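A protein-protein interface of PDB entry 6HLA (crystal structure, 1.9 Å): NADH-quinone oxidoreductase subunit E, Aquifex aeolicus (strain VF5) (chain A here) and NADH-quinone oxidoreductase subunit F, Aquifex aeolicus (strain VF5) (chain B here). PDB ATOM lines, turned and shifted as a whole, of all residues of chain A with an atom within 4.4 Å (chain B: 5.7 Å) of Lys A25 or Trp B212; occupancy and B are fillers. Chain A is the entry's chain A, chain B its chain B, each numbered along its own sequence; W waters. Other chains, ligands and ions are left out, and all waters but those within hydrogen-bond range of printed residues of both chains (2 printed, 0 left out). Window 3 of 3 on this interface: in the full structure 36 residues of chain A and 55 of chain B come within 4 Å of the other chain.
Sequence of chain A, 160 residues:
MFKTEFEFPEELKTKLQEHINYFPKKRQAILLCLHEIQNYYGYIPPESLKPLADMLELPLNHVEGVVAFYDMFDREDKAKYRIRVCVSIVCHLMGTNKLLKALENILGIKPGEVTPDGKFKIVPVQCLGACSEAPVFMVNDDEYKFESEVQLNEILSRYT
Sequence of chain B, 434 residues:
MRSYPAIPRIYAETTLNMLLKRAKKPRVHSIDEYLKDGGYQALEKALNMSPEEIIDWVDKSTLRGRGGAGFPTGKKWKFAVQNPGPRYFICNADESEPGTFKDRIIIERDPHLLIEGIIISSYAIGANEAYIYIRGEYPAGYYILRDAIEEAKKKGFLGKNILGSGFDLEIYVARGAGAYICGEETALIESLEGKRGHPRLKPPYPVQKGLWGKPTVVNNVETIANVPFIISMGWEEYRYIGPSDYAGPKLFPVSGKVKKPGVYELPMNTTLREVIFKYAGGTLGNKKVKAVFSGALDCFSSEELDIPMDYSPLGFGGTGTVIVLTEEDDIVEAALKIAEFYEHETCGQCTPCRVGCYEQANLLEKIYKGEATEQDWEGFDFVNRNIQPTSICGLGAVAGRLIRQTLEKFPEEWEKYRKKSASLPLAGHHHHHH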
ATOM      1  N   PHE A  23      19.982 -12.068  17.589  1.00  0.00           N
ATOM      2  CA  PHE A  23      19.647 -10.967  16.688  1.00  0.00           C
ATOM      3  C   PHE A  23      18.435 -10.223  17.191  1.00  0.00           C
ATOM      4  O   PHE A  23      17.626 -10.830  17.882  1.00  0.00           O
ATOM      5  CB  PHE A  23      19.393 -11.482  15.265  1.00  0.00           C
ATOM      6  CG  PHE A  23      20.606 -12.062  14.579  1.00  0.00           C
ATOM      7  CD1 PHE A  23      21.495 -11.244  13.890  1.00  0.00           C
ATOM      8  CD2 PHE A  23      20.863 -13.428  14.623  1.00  0.00           C
ATOM      9  CE1 PHE A  23      22.624 -11.781  13.262  1.00  0.00           C
ATOM     10  CE2 PHE A  23      21.989 -13.962  13.999  1.00  0.00           C
ATOM     11  CZ  PHE A  23      22.856 -13.135  13.309  1.00  0.00           C
ATOM     12  N   PRO A  24      18.259  -8.931  16.834  1.00  0.00           N
ATOM     13  CA  PRO A  24      17.065  -8.197  17.283  1.00  0.00           C
ATOM     14  C   PRO A  24      15.722  -8.841  16.890  1.00  0.00           C
ATOM     15  O   PRO A  24      14.762  -8.730  17.650  1.00  0.00           O
ATOM     16  CB  PRO A  24      17.256  -6.809  16.675  1.00  0.00           C
ATOM     17  CG  PRO A  24      18.714  -6.690  16.447  1.00  0.00           C
ATOM     18  CD  PRO A  24      19.148  -8.058  16.041  1.00  0.00           C
ATOM     19  N   LYS A  25      15.663  -9.533  15.726  1.00  0.00           N
ATOM     20  CA  LYS A  25      14.498 -10.273  15.251  1.00  0.00           C
ATOM     21  C   LYS A  25      14.817 -11.760  15.217  1.00  0.00           C
ATOM     22  O   LYS A  25      15.943 -12.129  14.902  1.00  0.00           O
ATOM     23  CB  LYS A  25      13.981  -9.739  13.898  1.00  0.00           C
ATOM     24  CG  LYS A  25      13.481  -8.295  14.001  1.00  0.00           C
ATOM     25  CD  LYS A  25      12.703  -7.814  12.785  1.00  0.00           C
ATOM     26  CE  LYS A  25      12.404  -6.337  12.903  1.00  0.00           C
ATOM     27  NZ  LYS A  25      11.931  -5.748  11.620  1.00  0.00           N
ATOM     28  N   LYS A  26      13.850 -12.614  15.609  1.00  0.00           N
ATOM     29  CA  LYS A  26      14.038 -14.078  15.682  1.00  0.00           C
ATOM     30  C   LYS A  26      14.387 -14.719  14.329  1.00  0.00           C
ATOM     31  O   LYS A  26      15.270 -15.577  14.270  1.00  0.00           O
ATOM     32  CB  LYS A  26      12.804 -14.775  16.299  1.00  0.00           C
ATOM     33  CG  LYS A  26      12.547 -14.468  17.776  1.00  0.00           C
ATOM     34  CD  LYS A  26      11.181 -14.975  18.195  1.00  0.00           C
ATOM     35  CE  LYS A  26      10.976 -14.969  19.689  1.00  0.00           C
ATOM     36  NZ  LYS A  26      11.021 -16.345  20.247  1.00  0.00           N
ATOM     37  N   ARG A  27      13.697 -14.287  13.246  1.00  0.00           N
ATOM     38  CA  ARG A  27      13.871 -14.821  11.886  1.00  0.00           C
ATOM     39  C   ARG A  27      15.273 -14.642  11.316  1.00  0.00           C
ATOM     40  O   ARG A  27      15.644 -15.379  10.395  1.00  0.00           O
ATOM     41  CB  ARG A  27      12.805 -14.293  10.910  1.00  0.00           C
ATOM     42  CG  ARG A  27      12.717 -12.785  10.707  1.00  0.00           C
ATOM     43  CD  ARG A  27      11.346 -12.498  10.126  1.00  0.00           C
ATOM     44  NE  ARG A  27      11.090 -11.090   9.809  1.00  0.00           N
ATOM     45  CZ  ARG A  27      10.608 -10.196  10.668  1.00  0.00           C
ATOM     46  NH1 ARG A  27      10.402 -10.526  11.936  1.00  0.00           N
ATOM     47  NH2 ARG A  27      10.361  -8.956  10.275  1.00  0.00           N
ATOM     48  N   GLN A  28      16.068 -13.719  11.895  1.00  0.00           N
ATOM     49  CA  GLN A  28      17.438 -13.437  11.468  1.00  0.00           C
ATOM     50  C   GLN A  28      18.413 -14.573  11.808  1.00  0.00           C
ATOM     51  O   GLN A  28      19.501 -14.622  11.244  1.00  0.00           O
ATOM     52  CB  GLN A  28      17.927 -12.116  12.079  1.00  0.00           C
ATOM     53  CG  GLN A  28      17.127 -10.891  11.651  1.00  0.00           C
ATOM     54  CD  GLN A  28      17.831  -9.628  12.056  1.00  0.00           C
ATOM     55  OE1 GLN A  28      17.616  -9.094  13.144  1.00  0.00           O
ATOM     56  NE2 GLN A  28      18.701  -9.124  11.195  1.00  0.00           N
ATOM     57  N   TYR B  88      21.295   1.710   9.538  1.00  0.00           N
ATOM     58  CA  TYR B  88      22.053   0.488   9.792  1.00  0.00           C
ATOM     59  C   TYR B  88      23.364   0.495   9.059  1.00  0.00           C
ATOM     60  O   TYR B  88      23.451   1.037   7.965  1.00  0.00           O
ATOM     61  CB  TYR B  88      21.250  -0.761   9.395  1.00  0.00           C
ATOM     62  CG  TYR B  88      19.966  -0.935  10.162  1.00  0.00           C
ATOM     63  CD1 TYR B  88      18.734  -0.885   9.514  1.00  0.00           C
ATOM     64  CD2 TYR B  88      19.975  -1.107  11.541  1.00  0.00           C
ATOM     65  CE1 TYR B  88      17.542  -1.025  10.218  1.00  0.00           C
ATOM     66  CE2 TYR B  88      18.790  -1.234  12.258  1.00  0.00           C
ATOM     67  CZ  TYR B  88      17.575  -1.196  11.592  1.00  0.00           C
ATOM     68  OH  TYR B  88      16.411  -1.327  12.310  1.00  0.00           O
ATOM     69  N   GLU B 129      23.074  -0.015  15.383  1.00  0.00           N
ATOM     70  CA  GLU B 129      23.036  -1.432  15.097  1.00  0.00           C
ATOM     71  C   GLU B 129      23.860  -1.678  13.846  1.00  0.00           C
ATOM     72  O   GLU B 129      23.576  -1.113  12.783  1.00  0.00           O
ATOM     73  CB  GLU B 129      21.563  -1.853  14.924  1.00  0.00           C
ATOM     74  CG  GLU B 129      21.285  -3.331  14.692  1.00  0.00           C
ATOM     75  CD  GLU B 129      19.803  -3.662  14.712  1.00  0.00           C
ATOM     76  OE1 GLU B 129      19.111  -3.212  15.654  1.00  0.00           O
ATOM     77  OE2 GLU B 129      19.326  -4.352  13.779  1.00  0.00           O
ATOM     78  N   TYR B 131      26.235  -4.803  11.519  1.00  0.00           N
ATOM     79  CA  TYR B 131      26.315  -6.227  11.225  1.00  0.00           C
ATOM     80  C   TYR B 131      27.600  -6.560  10.526  1.00  0.00           C
ATOM     81  O   TYR B 131      28.159  -5.721   9.834  1.00  0.00           O
ATOM     82  CB  TYR B 131      25.175  -6.629  10.262  1.00  0.00           C
ATOM     83  CG  TYR B 131      23.833  -6.667  10.936  1.00  0.00           C
ATOM     84  CD1 TYR B 131      23.069  -5.511  11.082  1.00  0.00           C
ATOM     85  CD2 TYR B 131      23.350  -7.845  11.498  1.00  0.00           C
ATOM     86  CE1 TYR B 131      21.849  -5.534  11.753  1.00  0.00           C
ATOM     87  CE2 TYR B 131      22.109  -7.886  12.129  1.00  0.00           C
ATOM     88  CZ  TYR B 131      21.374  -6.727  12.270  1.00  0.00           C
ATOM     89  OH  TYR B 131      20.165  -6.783  12.891  1.00  0.00           O
ATOM     90  N   ILE B 189      21.427  -8.170   2.415  1.00  0.00           N
ATOM     91  CA  ILE B 189      20.353  -7.587   3.251  1.00  0.00           C
ATOM     92  C   ILE B 189      19.153  -8.546   3.397  1.00  0.00           C
ATOM     93  O   ILE B 189      18.636  -8.697   4.508  1.00  0.00           O
ATOM     94  CB  ILE B 189      19.954  -6.185   2.748  1.00  0.00           C
ATOM     95  CG1 ILE B 189      21.076  -5.186   3.086  1.00  0.00           C
ATOM     96  CG2 ILE B 189      18.605  -5.705   3.347  1.00  0.00           C
ATOM     97  CD1 ILE B 189      21.087  -3.849   2.250  1.00  0.00           C
ATOM     98  N   LEU B 192      20.215 -11.262   5.671  1.00  0.00           N
ATOM     99  CA  LEU B 192      20.253 -10.700   7.033  1.00  0.00           C
ATOM    100  C   LEU B 192      18.863 -10.608   7.609  1.00  0.00           C
ATOM    101  O   LEU B 192      18.694 -10.595   8.830  1.00  0.00           O
ATOM    102  CB  LEU B 192      20.879  -9.310   7.021  1.00  0.00           C
ATOM    103  CG  LEU B 192      22.346  -9.194   7.416  1.00  0.00           C
ATOM    104  CD1 LEU B 192      22.738  -7.761   7.475  1.00  0.00           C
ATOM    105  CD2 LEU B 192      22.628  -9.867   8.735  1.00  0.00           C
ATOM    106  N   GLU B 193      17.858 -10.540   6.723  1.00  0.00           N
ATOM    107  CA  GLU B 193      16.441 -10.480   7.089  1.00  0.00           C
ATOM    108  C   GLU B 193      15.831 -11.886   7.281  1.00  0.00           C
ATOM    109  O   GLU B 193      14.670 -11.995   7.622  1.00  0.00           O
ATOM    110  CB  GLU B 193      15.661  -9.669   6.039  1.00  0.00           C
ATOM    111  CG  GLU B 193      15.900  -8.172   6.099  1.00  0.00           C
ATOM    112  CD  GLU B 193      15.170  -7.328   5.074  1.00  0.00           C
ATOM    113  OE1 GLU B 193      15.354  -6.093   5.100  1.00  0.00           O
ATOM    114  OE2 GLU B 193      14.407  -7.888   4.254  1.00  0.00           O
ATOM    115  N   GLY B 194      16.625 -12.934   7.081  1.00  0.00           N
ATOM    116  CA  GLY B 194      16.189 -14.317   7.258  1.00  0.00           C
ATOM    117  C   GLY B 194      15.577 -14.947   6.026  1.00  0.00           C
ATOM    118  O   GLY B 194      14.858 -15.946   6.120  1.00  0.00           O
ATOM    119  N   ARG B 200      17.695  -7.284  -4.923  1.00  0.00           N
ATOM    120  CA  ARG B 200      16.533  -6.407  -5.134  1.00  0.00           C
ATOM    121  C   ARG B 200      16.857  -5.492  -6.288  1.00  0.00           C
ATOM    122  O   ARG B 200      18.022  -5.181  -6.495  1.00  0.00           O
ATOM    123  CB  ARG B 200      16.324  -5.501  -3.904  1.00  0.00           C
ATOM    124  CG  ARG B 200      16.194  -6.224  -2.572  1.00  0.00           C
ATOM    125  CD  ARG B 200      16.116  -5.216  -1.451  1.00  0.00           C
ATOM    126  NE  ARG B 200      15.787  -5.856  -0.180  1.00  0.00           N
ATOM    127  CZ  ARG B 200      15.679  -5.217   0.982  1.00  0.00           C
ATOM    128  NH1 ARG B 200      15.874  -3.902   1.048  1.00  0.00           N
ATOM    129  NH2 ARG B 200      15.364  -5.883   2.085  1.00  0.00           N
ATOM    130  N   GLY B 210      17.147  -0.078   2.783  1.00  0.00           N
ATOM    131  CA  GLY B 210      17.986  -1.259   2.952  1.00  0.00           C
ATOM    132  C   GLY B 210      17.393  -2.272   3.886  1.00  0.00           C
ATOM    133  O   GLY B 210      16.312  -2.796   3.601  1.00  0.00           O
ATOM    134  N   LEU B 211      18.098  -2.532   5.027  1.00  0.00           N
ATOM    135  CA  LEU B 211      17.655  -3.454   6.075  1.00  0.00           C
ATOM    136  C   LEU B 211      16.393  -2.922   6.729  1.00  0.00           C
ATOM    137  O   LEU B 211      16.371  -1.795   7.228  1.00  0.00           O
ATOM    138  CB  LEU B 211      18.757  -3.699   7.124  1.00  0.00           C
ATOM    139  CG  LEU B 211      18.423  -4.716   8.239  1.00  0.00           C
ATOM    140  CD1 LEU B 211      18.425  -6.165   7.711  1.00  0.00           C
ATOM    141  CD2 LEU B 211      19.375  -4.570   9.419  1.00  0.00           C
ATOM    142  N   TRP B 212      15.315  -3.727   6.655  1.00  0.00           N
ATOM    143  CA  TRP B 212      13.975  -3.400   7.137  1.00  0.00           C
ATOM    144  C   TRP B 212      13.458  -2.107   6.464  1.00  0.00           C
ATOM    145  O   TRP B 212      12.662  -1.379   7.042  1.00  0.00           O
ATOM    146  CB  TRP B 212      13.905  -3.359   8.691  1.00  0.00           C
ATOM    147  CG  TRP B 212      14.592  -4.501   9.399  1.00  0.00           C
ATOM    148  CD1 TRP B 212      15.566  -4.403  10.346  1.00  0.00           C
ATOM    149  CD2 TRP B 212      14.301  -5.907   9.262  1.00  0.00           C
ATOM    150  NE1 TRP B 212      15.930  -5.658  10.786  1.00  0.00           N
ATOM    151  CE2 TRP B 212      15.178  -6.600  10.129  1.00  0.00           C
ATOM    152  CE3 TRP B 212      13.387  -6.647   8.483  1.00  0.00           C
ATOM    153  CZ2 TRP B 212      15.180  -7.996  10.231  1.00  0.00           C
ATOM    154  CZ3 TRP B 212      13.380  -8.028   8.598  1.00  0.00           C
ATOM    155  CH2 TRP B 212      14.251  -8.687   9.482  1.00  0.00           C
ATOM    156  N   GLY B 213      13.926  -1.849   5.238  1.00  0.00           N
ATOM    157  CA  GLY B 213      13.550  -0.672   4.456  1.00  0.00           C
ATOM    158  C   GLY B 213      14.134   0.648   4.937  1.00  0.00           C
ATOM    159  O   GLY B 213      13.758   1.713   4.435  1.00  0.00           O
ATOM    160  N   LYS B 214      15.092   0.582   5.891  1.00  0.00           N
ATOM    161  CA  LYS B 214      15.726   1.751   6.480  1.00  0.00           C
ATOM    162  C   LYS B 214      17.054   2.143   5.801  1.00  0.00           C
ATOM    163  O   LYS B 214      17.700   1.271   5.221  1.00  0.00           O
ATOM    164  CB  LYS B 214      15.917   1.525   8.007  1.00  0.00           C
ATOM    165  CG  LYS B 214      14.598   1.440   8.794  1.00  0.00           C
ATOM    166  CD  LYS B 214      13.956   2.822   8.980  1.00  0.00           C
ATOM    167  CE  LYS B 214      12.486   2.770   9.323  1.00  0.00           C
ATOM    168  NZ  LYS B 214      11.928   4.136   9.534  1.00  0.00           N
HETATM  169  O   HOH W   1      17.159  -6.267  13.228  1.00  0.00           O
HETATM  170  O   HOH W   2      12.252 -10.908   7.040  1.00  0.00           O
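Of the printed residues of chain B, Phe A23 touches Tyr B131.
Of the printed residues of chain B, Pro A24 touches Glu B129 (3.6 Å) and Tyr B131 (3.5 Å).
Tyr B88 touches none of the printed residues of chain A.
Of the printed residues of chain A, Glu B129 touches Pro A24 (3.6 Å).
Printed residues of chain A within 4 Å of Leu B192: Gln A28.
Of the printed residues of chain A, Glu B193 touches Arg A27 (3.7 Å).
Leu B211 touches none of the printed residues of chain A.
Trp B212 touches just these residues of chain A: Lys A25, Arg A27 and Gln A28.
The nearest printed residue of chain B that does not touch Lys A25 is Tyr B131 (6.0 Å).
OH of Tyr B131 is in hydrogen-bond range of NE2 of Gln A28.
O of Leu B192 is in hydrogen-bond range of NE2 of Gln A28, 2.8 Å away.
Phe A23 touches Tyr B131.
OE1 of Glu B129 touches CG of Pro A24, at 3.6 Å.
Tyr B131 touches Pro A24 (OH to CD, 3.5 Å).
Lys A25 touches Trp B212 (NZ to CD2, 3.3 Å).
Arg A27 touches Glu B193.
Arg A27 touches Gly B194.
Arg A27 touches Trp B212.
Trp B212 touches Gln A28 (CZ2 to CD, 3.6 Å).
Of the 13 printed residues of chain B, 6 touch a printed residue of chain A.
Printed residues of chain B that touch a printed residue of chain A: Glu B129, Tyr B131, Leu B192, Glu B193, Gly B194 and Trp B212.
Hydrophobic or aromatic side chains of chain B within 4 Å of the printed part of chain A: Tyr B131 and Trp B212.
Hydrophobic or aromatic side chains of chain A within 4 Å of the printed part of chain B: Phe A23 and Pro A24.
Along chain A the printed residues that touch a printed residue of chain B span positions 23 to 28.
Among the printed residues, 10 pairs touch across the chains.
OE1 of Gln A28 is in hydrogen-bond range of N of Lys A25.
OE2 of Glu B129 lies within hydrogen-bond range of OH of Tyr B131, 2.7 Å away.
The side-chain carboxylate (OE1) of Glu B193 lies within salt-bridge range of the guanidinium group (NH2) of Arg B200, 3.0 Å away.
OE1 of Glu B193 is in hydrogen-bond range of N of Trp B212, at 2.8 Å.
Water W2 bridges O of Glu B193 (2.7 Å) and NE of Arg A27 (3.0 Å).
Water W1 lies within hydrogen-bond range of NE1 of Trp B212 (2.8 Å), OE1 of Gln A28 (2.9 Å), OE2 of Glu B129 (2.9 Å) and OH of Tyr B131 (3.1 Å).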
